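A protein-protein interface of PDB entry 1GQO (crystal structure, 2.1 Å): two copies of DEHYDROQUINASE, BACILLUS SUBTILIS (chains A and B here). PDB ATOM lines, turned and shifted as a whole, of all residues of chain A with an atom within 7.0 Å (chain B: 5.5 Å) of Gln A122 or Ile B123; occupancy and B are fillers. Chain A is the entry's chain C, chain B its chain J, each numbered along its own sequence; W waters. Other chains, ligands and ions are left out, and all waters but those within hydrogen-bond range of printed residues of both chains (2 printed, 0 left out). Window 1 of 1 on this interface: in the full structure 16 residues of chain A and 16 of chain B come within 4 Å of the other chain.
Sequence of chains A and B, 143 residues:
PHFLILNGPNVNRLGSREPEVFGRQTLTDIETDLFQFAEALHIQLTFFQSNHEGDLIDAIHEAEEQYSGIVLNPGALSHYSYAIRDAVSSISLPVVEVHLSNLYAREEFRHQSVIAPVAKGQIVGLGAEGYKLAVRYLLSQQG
OH of Tyr A104 lies within hydrogen-bond range of OH of Tyr B104, 3.0 Å away. The backbone carbonyl oxygen (O) of Gln A122 sits at hydrogen-bond distance from the backbone NH (N) of Val B124 (3.0 Å). N of Val A124 is in hydrogen-bond range of O of Gln B122 (3.0 Å). O of Lys A120 lies close to O of Gly B125 (3.1 Å).
The backbone NH of Lys A120 is in hydrogen-bond range of the backbone carbonyl oxygen of Val A95 (3.0 Å). OE1 of Gln A122 sits close to OE2 of Glu A97 (3.2 Å). N of Ala A116 sits at hydrogen-bond distance from OG of Ser A113 (3.0 Å). The backbone carbonyl oxygen (O) of Gly B121 sits at hydrogen-bond distance from the backbone NH (N) of Glu B97 (3.2 Å). The side-chain amide oxygen (OE1) of Gln B122 lies close to the side-chain carboxylate (OE2) of Glu B97 (3.1 Å). The backbone NH of Gly B125 sits at hydrogen-bond distance from the backbone carbonyl oxygen of His B99.
CE1 of Tyr A104 touches NE2 of Gln B122, at 3.5 Å. Tyr B104 touches Ala A116. O of Val B124 touches CA of Gly A121, 3.2 Å away. Gly A121 touches Leu B126 (CA to CD2, 3.8 Å). O of Gln A122 touches CA of Ile B123, at 3.6 Å. Ile A123 touches Gln B122. Ile A123 touches Leu B126. O of Val A124 touches CA of Gly B121, at 3.1 Å. Gly B121 touches Leu A126 (CA to CD2, 3.8 Å). Ile B123 touches Leu A126.
Of the printed residues of chain B, Ala A116 touches Tyr B104. Gln A122 touches just these residues of chain B: Tyr B104 (3.6 Å), Ile B123 (3.6 Å) and Val B124 (3.0 Å). Printed residues of chain A within 4 Å of Tyr B104: Tyr A104, Ala A116 and Gln A122. Printed residues of chain A within 4 Å of Gly B121: Val A124 (3.1 Å) and Leu A126 (3.8 Å). Of chain A, only Gln A122 and Leu A126 come within 4 Å of Ile B123. Printed residues of chain A within 4 Å of Gly B125: Lys A120. Of the printed residues of chain A, Leu B126 touches Gly A121 and Ile A123. The nearest residue of chain B that does not touch Gln A122 is Gln B122 (4.1 Å). The nearest residue of chain A that does not touch Ile B123 is Ile A123 (4.2 Å). The nearest printed residue of chain B that does not touch Tyr A104 is Val B124 (5.9 Å).
Along chain B the printed residues that touch a printed residue of chain A span positions 104 to 133. Among the printed residues, 16 pairs touch across the chains.
Tyr A104 touches its own counterpart, Tyr B104. Tyr A104 touches Gln B122, and with the chains exchanged Gln A122 touches Tyr B104. Gly A121 touches Leu B126, and with the chains exchanged Leu A126 touches Gly B121. Ile A123 touches Leu B126, and with the chains exchanged Leu A126 touches Ile B123.
Water W1 lies within hydrogen-bond range of OH of Tyr B104 (2.7 Å), NE2 of Gln B122 (3.0 Å) and OH of Tyr A104 (3.4 Å). Water W2 bridges OH of Tyr A104 (3.4 Å) and OH of Tyr B104 (3.4 Å).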
ATOM      1  N   PRO A  74      28.118  -2.335  32.918  1.00  0.00           N
ATOM      2  CA  PRO A  74      29.350  -1.620  33.368  1.00  0.00           C
ATOM      3  C   PRO A  74      29.626  -0.392  32.585  1.00  0.00           C
ATOM      4  O   PRO A  74      30.708   0.112  32.750  1.00  0.00           O
ATOM      5  CB  PRO A  74      30.481  -2.633  33.127  1.00  0.00           C
ATOM      6  CG  PRO A  74      29.931  -3.317  31.922  1.00  0.00           C
ATOM      7  CD  PRO A  74      28.473  -3.502  32.119  1.00  0.00           C
ATOM      8  N   SER A  78      33.133  -1.905  30.124  1.00  0.00           N
ATOM      9  CA  SER A  78      33.032  -3.146  29.380  1.00  0.00           C
ATOM     10  C   SER A  78      34.229  -3.398  28.380  1.00  0.00           C
ATOM     11  O   SER A  78      34.718  -4.533  28.128  1.00  0.00           O
ATOM     12  CB  SER A  78      31.812  -3.150  28.414  1.00  0.00           C
ATOM     13  OG  SER A  78      31.734  -4.430  27.763  1.00  0.00           O
ATOM     14  N   HIS A  79      34.730  -2.295  27.835  1.00  0.00           N
ATOM     15  CA  HIS A  79      35.721  -2.343  26.797  1.00  0.00           C
ATOM     16  C   HIS A  79      37.167  -2.448  27.170  1.00  0.00           C
ATOM     17  O   HIS A  79      38.034  -2.537  26.276  1.00  0.00           O
ATOM     18  CB  HIS A  79      35.457  -1.305  25.696  1.00  0.00           C
ATOM     19  CG  HIS A  79      33.966  -1.156  25.460  1.00  0.00           C
ATOM     20  ND1 HIS A  79      33.209  -2.226  25.057  1.00  0.00           N
ATOM     21  CD2 HIS A  79      33.140  -0.070  25.669  1.00  0.00           C
ATOM     22  CE1 HIS A  79      31.934  -1.810  25.000  1.00  0.00           C
ATOM     23  NE2 HIS A  79      31.879  -0.525  25.369  1.00  0.00           N
ATOM     24  N   VAL A  95      26.593 -14.084  36.435  1.00  0.00           N
ATOM     25  CA  VAL A  95      26.626 -12.713  36.029  1.00  0.00           C
ATOM     26  C   VAL A  95      26.245 -12.615  34.561  1.00  0.00           C
ATOM     27  O   VAL A  95      26.696 -13.386  33.700  1.00  0.00           O
ATOM     28  CB  VAL A  95      28.042 -12.116  36.163  1.00  0.00           C
ATOM     29  CG1 VAL A  95      28.219 -10.687  35.768  1.00  0.00           C
ATOM     30  CG2 VAL A  95      28.547 -12.337  37.602  1.00  0.00           C
ATOM     31  N   VAL A  96      25.238 -11.758  34.271  1.00  0.00           N
ATOM     32  CA  VAL A  96      24.885 -11.447  32.889  1.00  0.00           C
ATOM     33  C   VAL A  96      25.238  -9.984  32.590  1.00  0.00           C
ATOM     34  O   VAL A  96      24.887  -9.064  33.325  1.00  0.00           O
ATOM     35  CB  VAL A  96      23.433 -11.721  32.543  1.00  0.00           C
ATOM     36  CG1 VAL A  96      23.071 -11.502  31.073  1.00  0.00           C
ATOM     37  CG2 VAL A  96      22.992 -13.110  32.950  1.00  0.00           C
ATOM     38  N   GLU A  97      25.981  -9.803  31.498  1.00  0.00           N
ATOM     39  CA  GLU A  97      26.347  -8.434  31.093  1.00  0.00           C
ATOM     40  C   GLU A  97      25.237  -7.822  30.215  1.00  0.00           C
ATOM     41  O   GLU A  97      24.782  -8.488  29.313  1.00  0.00           O
ATOM     42  CB  GLU A  97      27.698  -8.376  30.409  1.00  0.00           C
ATOM     43  CG  GLU A  97      28.194  -6.953  30.095  1.00  0.00           C
ATOM     44  CD  GLU A  97      29.545  -6.851  29.399  1.00  0.00           C
ATOM     45  OE1 GLU A  97      30.061  -5.693  29.261  1.00  0.00           O
ATOM     46  OE2 GLU A  97      30.191  -7.870  29.066  1.00  0.00           O
ATOM     47  N   VAL A  98      24.734  -6.650  30.563  1.00  0.00           N
ATOM     48  CA  VAL A  98      23.686  -6.015  29.766  1.00  0.00           C
ATOM     49  C   VAL A  98      23.985  -4.618  29.243  1.00  0.00           C
ATOM     50  O   VAL A  98      24.598  -3.794  29.915  1.00  0.00           O
ATOM     51  CB  VAL A  98      22.387  -5.970  30.645  1.00  0.00           C
ATOM     52  CG1 VAL A  98      21.290  -5.233  29.918  1.00  0.00           C
ATOM     53  CG2 VAL A  98      21.936  -7.424  30.833  1.00  0.00           C
ATOM     54  N   HIS A  99      23.639  -4.237  28.041  1.00  0.00           N
ATOM     55  CA  HIS A  99      23.792  -2.977  27.403  1.00  0.00           C
ATOM     56  C   HIS A  99      22.477  -2.660  26.659  1.00  0.00           C
ATOM     57  O   HIS A  99      21.980  -3.488  25.876  1.00  0.00           O
ATOM     58  CB  HIS A  99      24.980  -2.800  26.453  1.00  0.00           C
ATOM     59  CG  HIS A  99      26.259  -3.026  27.138  1.00  0.00           C
ATOM     60  ND1 HIS A  99      26.955  -2.059  27.808  1.00  0.00           N
ATOM     61  CD2 HIS A  99      26.974  -4.157  27.369  1.00  0.00           C
ATOM     62  CE1 HIS A  99      28.031  -2.563  28.354  1.00  0.00           C
ATOM     63  NE2 HIS A  99      28.080  -3.858  28.109  1.00  0.00           N
ATOM     64  N   LEU A 103      25.473  -1.754  20.662  1.00  0.00           N
ATOM     65  CA  LEU A 103      26.819  -1.352  20.627  1.00  0.00           C
ATOM     66  C   LEU A 103      27.493  -1.570  19.291  1.00  0.00           C
ATOM     67  O   LEU A 103      28.260  -0.683  18.902  1.00  0.00           O
ATOM     68  CB  LEU A 103      27.638  -2.129  21.689  1.00  0.00           C
ATOM     69  CG  LEU A 103      27.196  -1.962  23.126  1.00  0.00           C
ATOM     70  CD1 LEU A 103      28.127  -2.577  24.120  1.00  0.00           C
ATOM     71  CD2 LEU A 103      26.983  -0.468  23.453  1.00  0.00           C
ATOM     72  N   TYR A 104      27.167  -2.630  18.589  1.00  0.00           N
ATOM     73  CA  TYR A 104      27.705  -3.023  17.332  1.00  0.00           C
ATOM     74  C   TYR A 104      27.427  -2.101  16.190  1.00  0.00           C
ATOM     75  O   TYR A 104      28.121  -2.208  15.173  1.00  0.00           O
ATOM     76  CB  TYR A 104      27.174  -4.446  17.021  1.00  0.00           C
ATOM     77  CG  TYR A 104      27.433  -5.417  18.139  1.00  0.00           C
ATOM     78  CD1 TYR A 104      26.380  -6.159  18.752  1.00  0.00           C
ATOM     79  CD2 TYR A 104      28.694  -5.626  18.635  1.00  0.00           C
ATOM     80  CE1 TYR A 104      26.641  -7.034  19.791  1.00  0.00           C
ATOM     81  CE2 TYR A 104      28.948  -6.472  19.683  1.00  0.00           C
ATOM     82  CZ  TYR A 104      27.922  -7.223  20.226  1.00  0.00           C
ATOM     83  OH  TYR A 104      28.293  -8.034  21.286  1.00  0.00           O
ATOM     84  N   ARG A 110      33.517  -0.012  21.003  1.00  0.00           N
ATOM     85  CA  ARG A 110      32.411  -0.640  21.771  1.00  0.00           C
ATOM     86  C   ARG A 110      32.013  -1.981  21.336  1.00  0.00           C
ATOM     87  O   ARG A 110      31.195  -2.604  21.993  1.00  0.00           O
ATOM     88  CB  ARG A 110      31.146   0.217  21.851  1.00  0.00           C
ATOM     89  CG  ARG A 110      31.296   1.681  22.165  1.00  0.00           C
ATOM     90  CD  ARG A 110      29.876   2.335  22.122  1.00  0.00           C
ATOM     91  NE  ARG A 110      30.023   3.751  22.301  1.00  0.00           N
ATOM     92  CZ  ARG A 110      30.355   4.444  23.372  1.00  0.00           C
ATOM     93  NH1 ARG A 110      30.502   3.890  24.574  1.00  0.00           N
ATOM     94  NH2 ARG A 110      30.520   5.766  23.285  1.00  0.00           N
ATOM     95  N   HIS A 111      32.593  -2.567  20.318  1.00  0.00           N
ATOM     96  CA  HIS A 111      32.284  -3.857  19.780  1.00  0.00           C
ATOM     97  C   HIS A 111      32.914  -5.038  20.503  1.00  0.00           C
ATOM     98  O   HIS A 111      32.550  -6.131  20.135  1.00  0.00           O
ATOM     99  CB  HIS A 111      32.646  -3.934  18.317  1.00  0.00           C
ATOM    100  CG  HIS A 111      31.957  -2.910  17.465  1.00  0.00           C
ATOM    101  ND1 HIS A 111      31.999  -3.022  16.094  1.00  0.00           N
ATOM    102  CD2 HIS A 111      31.199  -1.846  17.735  1.00  0.00           C
ATOM    103  CE1 HIS A 111      31.364  -1.958  15.583  1.00  0.00           C
ATOM    104  NE2 HIS A 111      30.828  -1.258  16.569  1.00  0.00           N
ATOM    105  N   GLN A 112      33.646  -4.887  21.549  1.00  0.00           N
ATOM    106  CA  GLN A 112      34.243  -5.982  22.266  1.00  0.00           C
ATOM    107  C   GLN A 112      34.072  -5.711  23.759  1.00  0.00           C
ATOM    108  O   GLN A 112      34.189  -4.571  24.183  1.00  0.00           O
ATOM    109  CB  GLN A 112      35.736  -6.172  22.010  1.00  0.00           C
ATOM    110  CG  GLN A 112      36.709  -5.799  23.076  1.00  0.00           C
ATOM    111  CD  GLN A 112      37.430  -4.536  23.415  1.00  0.00           C
ATOM    112  OE1 GLN A 112      38.466  -4.516  24.144  1.00  0.00           O
ATOM    113  NE2 GLN A 112      37.075  -3.320  22.963  1.00  0.00           N
ATOM    114  N   SER A 113      33.803  -6.771  24.509  1.00  0.00           N
ATOM    115  CA  SER A 113      33.710  -6.715  25.921  1.00  0.00           C
ATOM    116  C   SER A 113      34.827  -7.617  26.469  1.00  0.00           C
ATOM    117  O   SER A 113      34.913  -8.779  25.999  1.00  0.00           O
ATOM    118  CB  SER A 113      32.400  -7.308  26.500  1.00  0.00           C
ATOM    119  OG  SER A 113      32.550  -7.453  27.891  1.00  0.00           O
ATOM    120  N   ILE A 115      34.751  -8.393  29.641  1.00  0.00           N
ATOM    121  CA  ILE A 115      34.066  -9.030  30.745  1.00  0.00           C
ATOM    122  C   ILE A 115      33.277 -10.235  30.328  1.00  0.00           C
ATOM    123  O   ILE A 115      33.205 -11.288  31.000  1.00  0.00           O
ATOM    124  CB  ILE A 115      33.091  -8.078  31.459  1.00  0.00           C
ATOM    125  CG1 ILE A 115      33.869  -6.936  32.116  1.00  0.00           C
ATOM    126  CG2 ILE A 115      32.312  -8.754  32.603  1.00  0.00           C
ATOM    127  CD1 ILE A 115      33.058  -5.711  32.457  1.00  0.00           C
ATOM    128  N   ALA A 116      32.772 -10.184  29.082  1.00  0.00           N
ATOM    129  CA  ALA A 116      31.891 -11.245  28.596  1.00  0.00           C
ATOM    130  C   ALA A 116      32.433 -12.651  28.568  1.00  0.00           C
ATOM    131  O   ALA A 116      31.707 -13.606  28.877  1.00  0.00           O
ATOM    132  CB  ALA A 116      31.254 -10.935  27.231  1.00  0.00           C
ATOM    133  N   ALA A 119      31.692 -14.264  31.862  1.00  0.00           N
ATOM    134  CA  ALA A 119      30.325 -14.188  32.423  1.00  0.00           C
ATOM    135  C   ALA A 119      29.503 -15.306  31.800  1.00  0.00           C
ATOM    136  O   ALA A 119      30.032 -16.090  30.973  1.00  0.00           O
ATOM    137  CB  ALA A 119      29.813 -12.804  32.092  1.00  0.00           C
ATOM    138  N   LYS A 120      28.274 -15.449  32.252  1.00  0.00           N
ATOM    139  CA  LYS A 120      27.364 -16.442  31.662  1.00  0.00           C
ATOM    140  C   LYS A 120      27.090 -16.003  30.241  1.00  0.00           C
ATOM    141  O   LYS A 120      27.064 -16.789  29.296  1.00  0.00           O
ATOM    142  CB  LYS A 120      26.044 -16.520  32.460  1.00  0.00           C
ATOM    143  CG  LYS A 120      26.223 -17.190  33.845  1.00  0.00           C
ATOM    144  CD  LYS A 120      26.159 -18.660  33.470  1.00  0.00           C
ATOM    145  CE  LYS A 120      26.960 -19.535  34.380  1.00  0.00           C
ATOM    146  NZ  LYS A 120      26.998 -20.872  33.717  1.00  0.00           N
ATOM    147  N   GLY A 121      26.844 -14.677  30.045  1.00  0.00           N
ATOM    148  CA  GLY A 121      26.478 -14.332  28.602  1.00  0.00           C
ATOM    149  C   GLY A 121      26.304 -12.781  28.637  1.00  0.00           C
ATOM    150  O   GLY A 121      26.583 -12.173  29.662  1.00  0.00           O
ATOM    151  N   GLN A 122      25.661 -12.328  27.570  1.00  0.00           N
ATOM    152  CA  GLN A 122      25.490 -10.925  27.366  1.00  0.00           C
ATOM    153  C   GLN A 122      24.282 -10.625  26.512  1.00  0.00           C
ATOM    154  O   GLN A 122      23.922 -11.475  25.667  1.00  0.00           O
ATOM    155  CB  GLN A 122      26.802 -10.394  26.656  1.00  0.00           C
ATOM    156  CG  GLN A 122      26.858  -8.968  26.376  1.00  0.00           C
ATOM    157  CD  GLN A 122      28.101  -8.288  25.804  1.00  0.00           C
ATOM    158  OE1 GLN A 122      28.585  -7.318  26.387  1.00  0.00           O
ATOM    159  NE2 GLN A 122      28.595  -8.719  24.649  1.00  0.00           N
ATOM    160  N   ILE A 123      23.574  -9.561  26.814  1.00  0.00           N
ATOM    161  CA  ILE A 123      22.464  -9.091  25.997  1.00  0.00           C
ATOM    162  C   ILE A 123      22.755  -7.663  25.560  1.00  0.00           C
ATOM    163  O   ILE A 123      22.918  -6.813  26.425  1.00  0.00           O
ATOM    164  CB  ILE A 123      21.143  -9.034  26.800  1.00  0.00           C
ATOM    165  CG1 ILE A 123      20.801 -10.443  27.285  1.00  0.00           C
ATOM    166  CG2 ILE A 123      20.024  -8.576  25.884  1.00  0.00           C
ATOM    167  CD1 ILE A 123      19.721 -10.487  28.345  1.00  0.00           C
ATOM    168  N   VAL A 124      22.774  -7.422  24.249  1.00  0.00           N
ATOM    169  CA  VAL A 124      23.019  -6.082  23.780  1.00  0.00           C
ATOM    170  C   VAL A 124      21.955  -5.539  22.858  1.00  0.00           C
ATOM    171  O   VAL A 124      21.550  -6.240  21.933  1.00  0.00           O
ATOM    172  CB  VAL A 124      24.315  -6.135  22.976  1.00  0.00           C
ATOM    173  CG1 VAL A 124      24.521  -4.858  22.204  1.00  0.00           C
ATOM    174  CG2 VAL A 124      25.529  -6.280  23.870  1.00  0.00           C
ATOM    175  N   LEU A 126      18.802  -4.510  23.301  1.00  0.00           N
ATOM    176  CA  LEU A 126      17.394  -4.699  23.540  1.00  0.00           C
ATOM    177  C   LEU A 126      16.755  -3.699  24.470  1.00  0.00           C
ATOM    178  O   LEU A 126      15.658  -3.923  24.940  1.00  0.00           O
ATOM    179  CB  LEU A 126      17.228  -6.134  23.971  1.00  0.00           C
ATOM    180  CG  LEU A 126      17.749  -7.169  22.983  1.00  0.00           C
ATOM    181  CD1 LEU A 126      17.344  -8.562  23.445  1.00  0.00           C
ATOM    182  CD2 LEU A 126      17.278  -6.985  21.537  1.00  0.00           C
ATOM    183  N   LEU A 133      15.020  -9.340  30.780  1.00  0.00           N
ATOM    184  CA  LEU A 133      15.389 -10.619  30.159  1.00  0.00           C
ATOM    185  C   LEU A 133      16.521 -11.276  30.966  1.00  0.00           C
ATOM    186  O   LEU A 133      16.615 -12.515  31.102  1.00  0.00           O
ATOM    187  CB  LEU A 133      15.719 -10.367  28.727  1.00  0.00           C
ATOM    188  CG  LEU A 133      14.633  -9.710  27.871  1.00  0.00           C
ATOM    189  CD1 LEU A 133      15.112  -9.475  26.461  1.00  0.00           C
ATOM    190  CD2 LEU A 133      13.396 -10.593  27.853  1.00  0.00           C
ATOM    191  N   VAL B  96      16.385 -10.466  15.862  1.00  0.00           N
ATOM    192  CA  VAL B  96      17.157 -10.627  17.072  1.00  0.00           C
ATOM    193  C   VAL B  96      18.105 -11.789  16.793  1.00  0.00           C
ATOM    194  O   VAL B  96      17.637 -12.912  16.472  1.00  0.00           O
ATOM    195  CB  VAL B  96      16.421 -10.903  18.390  1.00  0.00           C
ATOM    196  CG1 VAL B  96      17.403 -10.946  19.566  1.00  0.00           C
ATOM    197  CG2 VAL B  96      15.468  -9.797  18.716  1.00  0.00           C
ATOM    198  N   GLU B  97      19.406 -11.620  16.906  1.00  0.00           N
ATOM    199  CA  GLU B  97      20.382 -12.664  16.725  1.00  0.00           C
ATOM    200  C   GLU B  97      20.594 -13.391  18.047  1.00  0.00           C
ATOM    201  O   GLU B  97      20.740 -12.737  19.102  1.00  0.00           O
ATOM    202  CB  GLU B  97      21.738 -12.129  16.214  1.00  0.00           C
ATOM    203  CG  GLU B  97      22.692 -13.272  15.888  1.00  0.00           C
ATOM    204  CD  GLU B  97      24.014 -12.781  15.281  1.00  0.00           C
ATOM    205  OE1 GLU B  97      24.860 -13.559  14.815  1.00  0.00           O
ATOM    206  OE2 GLU B  97      24.229 -11.588  15.260  1.00  0.00           O
ATOM    207  N   VAL B  98      20.652 -14.683  18.066  1.00  0.00           N
ATOM    208  CA  VAL B  98      20.763 -15.506  19.240  1.00  0.00           C
ATOM    209  C   VAL B  98      21.729 -16.642  19.063  1.00  0.00           C
ATOM    210  O   VAL B  98      21.799 -17.292  18.021  1.00  0.00           O
ATOM    211  CB  VAL B  98      19.346 -16.115  19.567  1.00  0.00           C
ATOM    212  CG1 VAL B  98      19.553 -17.167  20.654  1.00  0.00           C
ATOM    213  CG2 VAL B  98      18.346 -15.094  20.065  1.00  0.00           C
ATOM    214  N   HIS B  99      22.644 -16.893  19.997  1.00  0.00           N
ATOM    215  CA  HIS B  99      23.580 -17.943  20.044  1.00  0.00           C
ATOM    216  C   HIS B  99      23.503 -18.622  21.437  1.00  0.00           C
ATOM    217  O   HIS B  99      23.558 -17.841  22.360  1.00  0.00           O
ATOM    218  CB  HIS B  99      25.095 -17.511  19.901  1.00  0.00           C
ATOM    219  CG  HIS B  99      25.282 -16.973  18.530  1.00  0.00           C
ATOM    220  ND1 HIS B  99      25.597 -17.798  17.479  1.00  0.00           N
ATOM    221  CD2 HIS B  99      25.070 -15.746  18.011  1.00  0.00           C
ATOM    222  CE1 HIS B  99      25.599 -17.057  16.397  1.00  0.00           C
ATOM    223  NE2 HIS B  99      25.272 -15.790  16.676  1.00  0.00           N
ATOM    224  N   TYR B 104      32.127 -15.697  23.368  1.00  0.00           N
ATOM    225  CA  TYR B 104      33.204 -14.929  23.921  1.00  0.00           C
ATOM    226  C   TYR B 104      34.190 -15.763  24.690  1.00  0.00           C
ATOM    227  O   TYR B 104      35.359 -15.398  24.700  1.00  0.00           O
ATOM    228  CB  TYR B 104      32.640 -13.749  24.728  1.00  0.00           C
ATOM    229  CG  TYR B 104      31.644 -12.961  23.894  1.00  0.00           C
ATOM    230  CD1 TYR B 104      30.361 -12.775  24.355  1.00  0.00           C
ATOM    231  CD2 TYR B 104      31.966 -12.453  22.658  1.00  0.00           C
ATOM    232  CE1 TYR B 104      29.433 -12.042  23.604  1.00  0.00           C
ATOM    233  CE2 TYR B 104      31.034 -11.773  21.901  1.00  0.00           C
ATOM    234  CZ  TYR B 104      29.769 -11.579  22.381  1.00  0.00           C
ATOM    235  OH  TYR B 104      28.895 -10.908  21.570  1.00  0.00           O
ATOM    236  N   GLY B 121      19.307  -6.453  18.121  1.00  0.00           N
ATOM    237  CA  GLY B 121      20.226  -6.721  19.225  1.00  0.00           C
ATOM    238  C   GLY B 121      20.688  -8.169  19.113  1.00  0.00           C
ATOM    239  O   GLY B 121      20.376  -8.785  18.122  1.00  0.00           O
ATOM    240  N   GLN B 122      21.394  -8.633  20.085  1.00  0.00           N
ATOM    241  CA  GLN B 122      21.922  -9.965  20.118  1.00  0.00           C
ATOM    242  C   GLN B 122      21.916 -10.496  21.573  1.00  0.00           C
ATOM    243  O   GLN B 122      22.104  -9.730  22.481  1.00  0.00           O
ATOM    244  CB  GLN B 122      23.375  -9.975  19.599  1.00  0.00           C
ATOM    245  CG  GLN B 122      24.065 -11.338  19.585  1.00  0.00           C
ATOM    246  CD  GLN B 122      25.419 -11.350  18.868  1.00  0.00           C
ATOM    247  OE1 GLN B 122      25.629 -12.154  17.935  1.00  0.00           O
ATOM    248  NE2 GLN B 122      26.349 -10.520  19.319  1.00  0.00           N
ATOM    249  N   ILE B 123      21.736 -11.814  21.743  1.00  0.00           N
ATOM    250  CA  ILE B 123      21.755 -12.512  23.026  1.00  0.00           C
ATOM    251  C   ILE B 123      22.690 -13.706  22.862  1.00  0.00           C
ATOM    252  O   ILE B 123      22.611 -14.454  21.881  1.00  0.00           O
ATOM    253  CB  ILE B 123      20.423 -13.133  23.469  1.00  0.00           C
ATOM    254  CG1 ILE B 123      19.360 -12.051  23.543  1.00  0.00           C
ATOM    255  CG2 ILE B 123      20.557 -13.860  24.791  1.00  0.00           C
ATOM    256  CD1 ILE B 123      17.975 -12.441  23.930  1.00  0.00           C
ATOM    257  N   VAL B 124      23.732 -13.747  23.701  1.00  0.00           N
ATOM    258  CA  VAL B 124      24.709 -14.794  23.490  1.00  0.00           C
ATOM    259  C   VAL B 124      24.967 -15.474  24.831  1.00  0.00           C
ATOM    260  O   VAL B 124      25.154 -14.690  25.764  1.00  0.00           O
ATOM    261  CB  VAL B 124      26.020 -14.095  23.076  1.00  0.00           C
ATOM    262  CG1 VAL B 124      27.222 -15.033  23.146  1.00  0.00           C
ATOM    263  CG2 VAL B 124      25.980 -13.478  21.741  1.00  0.00           C
ATOM    264  N   GLY B 125      25.164 -16.771  24.840  1.00  0.00           N
ATOM    265  CA  GLY B 125      25.577 -17.379  26.144  1.00  0.00           C
ATOM    266  C   GLY B 125      24.495 -17.844  27.090  1.00  0.00           C
ATOM    267  O   GLY B 125      24.730 -18.507  28.099  1.00  0.00           O
ATOM    268  N   LEU B 126      23.183 -17.528  26.814  1.00  0.00           N
ATOM    269  CA  LEU B 126      22.133 -17.887  27.758  1.00  0.00           C
ATOM    270  C   LEU B 126      21.409 -19.167  27.463  1.00  0.00           C
ATOM    271  O   LEU B 126      20.348 -19.318  27.985  1.00  0.00           O
ATOM    272  CB  LEU B 126      21.202 -16.664  27.877  1.00  0.00           C
ATOM    273  CG  LEU B 126      21.893 -15.395  28.130  1.00  0.00           C
ATOM    274  CD1 LEU B 126      20.925 -14.230  28.413  1.00  0.00           C
ATOM    275  CD2 LEU B 126      22.870 -15.456  29.318  1.00  0.00           C
ATOM    276  N   GLY B 130      17.591 -18.267  25.529  1.00  0.00           N
ATOM    277  CA  GLY B 130      17.815 -17.146  24.665  1.00  0.00           C
ATOM    278  C   GLY B 130      16.748 -17.007  23.589  1.00  0.00           C
ATOM    279  O   GLY B 130      16.347 -15.872  23.254  1.00  0.00           O
ATOM    280  N   LEU B 133      13.781 -15.541  25.384  1.00  0.00           N
ATOM    281  CA  LEU B 133      14.079 -14.154  25.699  1.00  0.00           C
ATOM    282  C   LEU B 133      13.905 -13.327  24.475  1.00  0.00           C
ATOM    283  O   LEU B 133      13.329 -12.251  24.483  1.00  0.00           O
ATOM    284  CB  LEU B 133      15.457 -14.020  26.373  1.00  0.00           C
ATOM    285  CG  LEU B 133      15.666 -14.861  27.654  1.00  0.00           C
ATOM    286  CD1 LEU B 133      17.102 -14.589  28.075  1.00  0.00           C
ATOM    287  CD2 LEU B 133      14.734 -14.464  28.744  1.00  0.00           C
ATOM    288  N   ALA B 134      14.390 -13.821  23.325  1.00  0.00           N
ATOM    289  CA  ALA B 134      14.251 -13.028  22.092  1.00  0.00           C
ATOM    290  C   ALA B 134      12.760 -12.839  21.674  1.00  0.00           C
ATOM    291  O   ALA B 134      12.339 -11.778  21.271  1.00  0.00           O
ATOM    292  CB  ALA B 134      14.994 -13.627  20.928  1.00  0.00           C
HETATM  293  O   HOH W   1      29.346 -10.218  18.970  1.00  0.00           O
HETATM  294  O   HOH W   2      25.853  -9.833  22.726  1.00  0.00           O
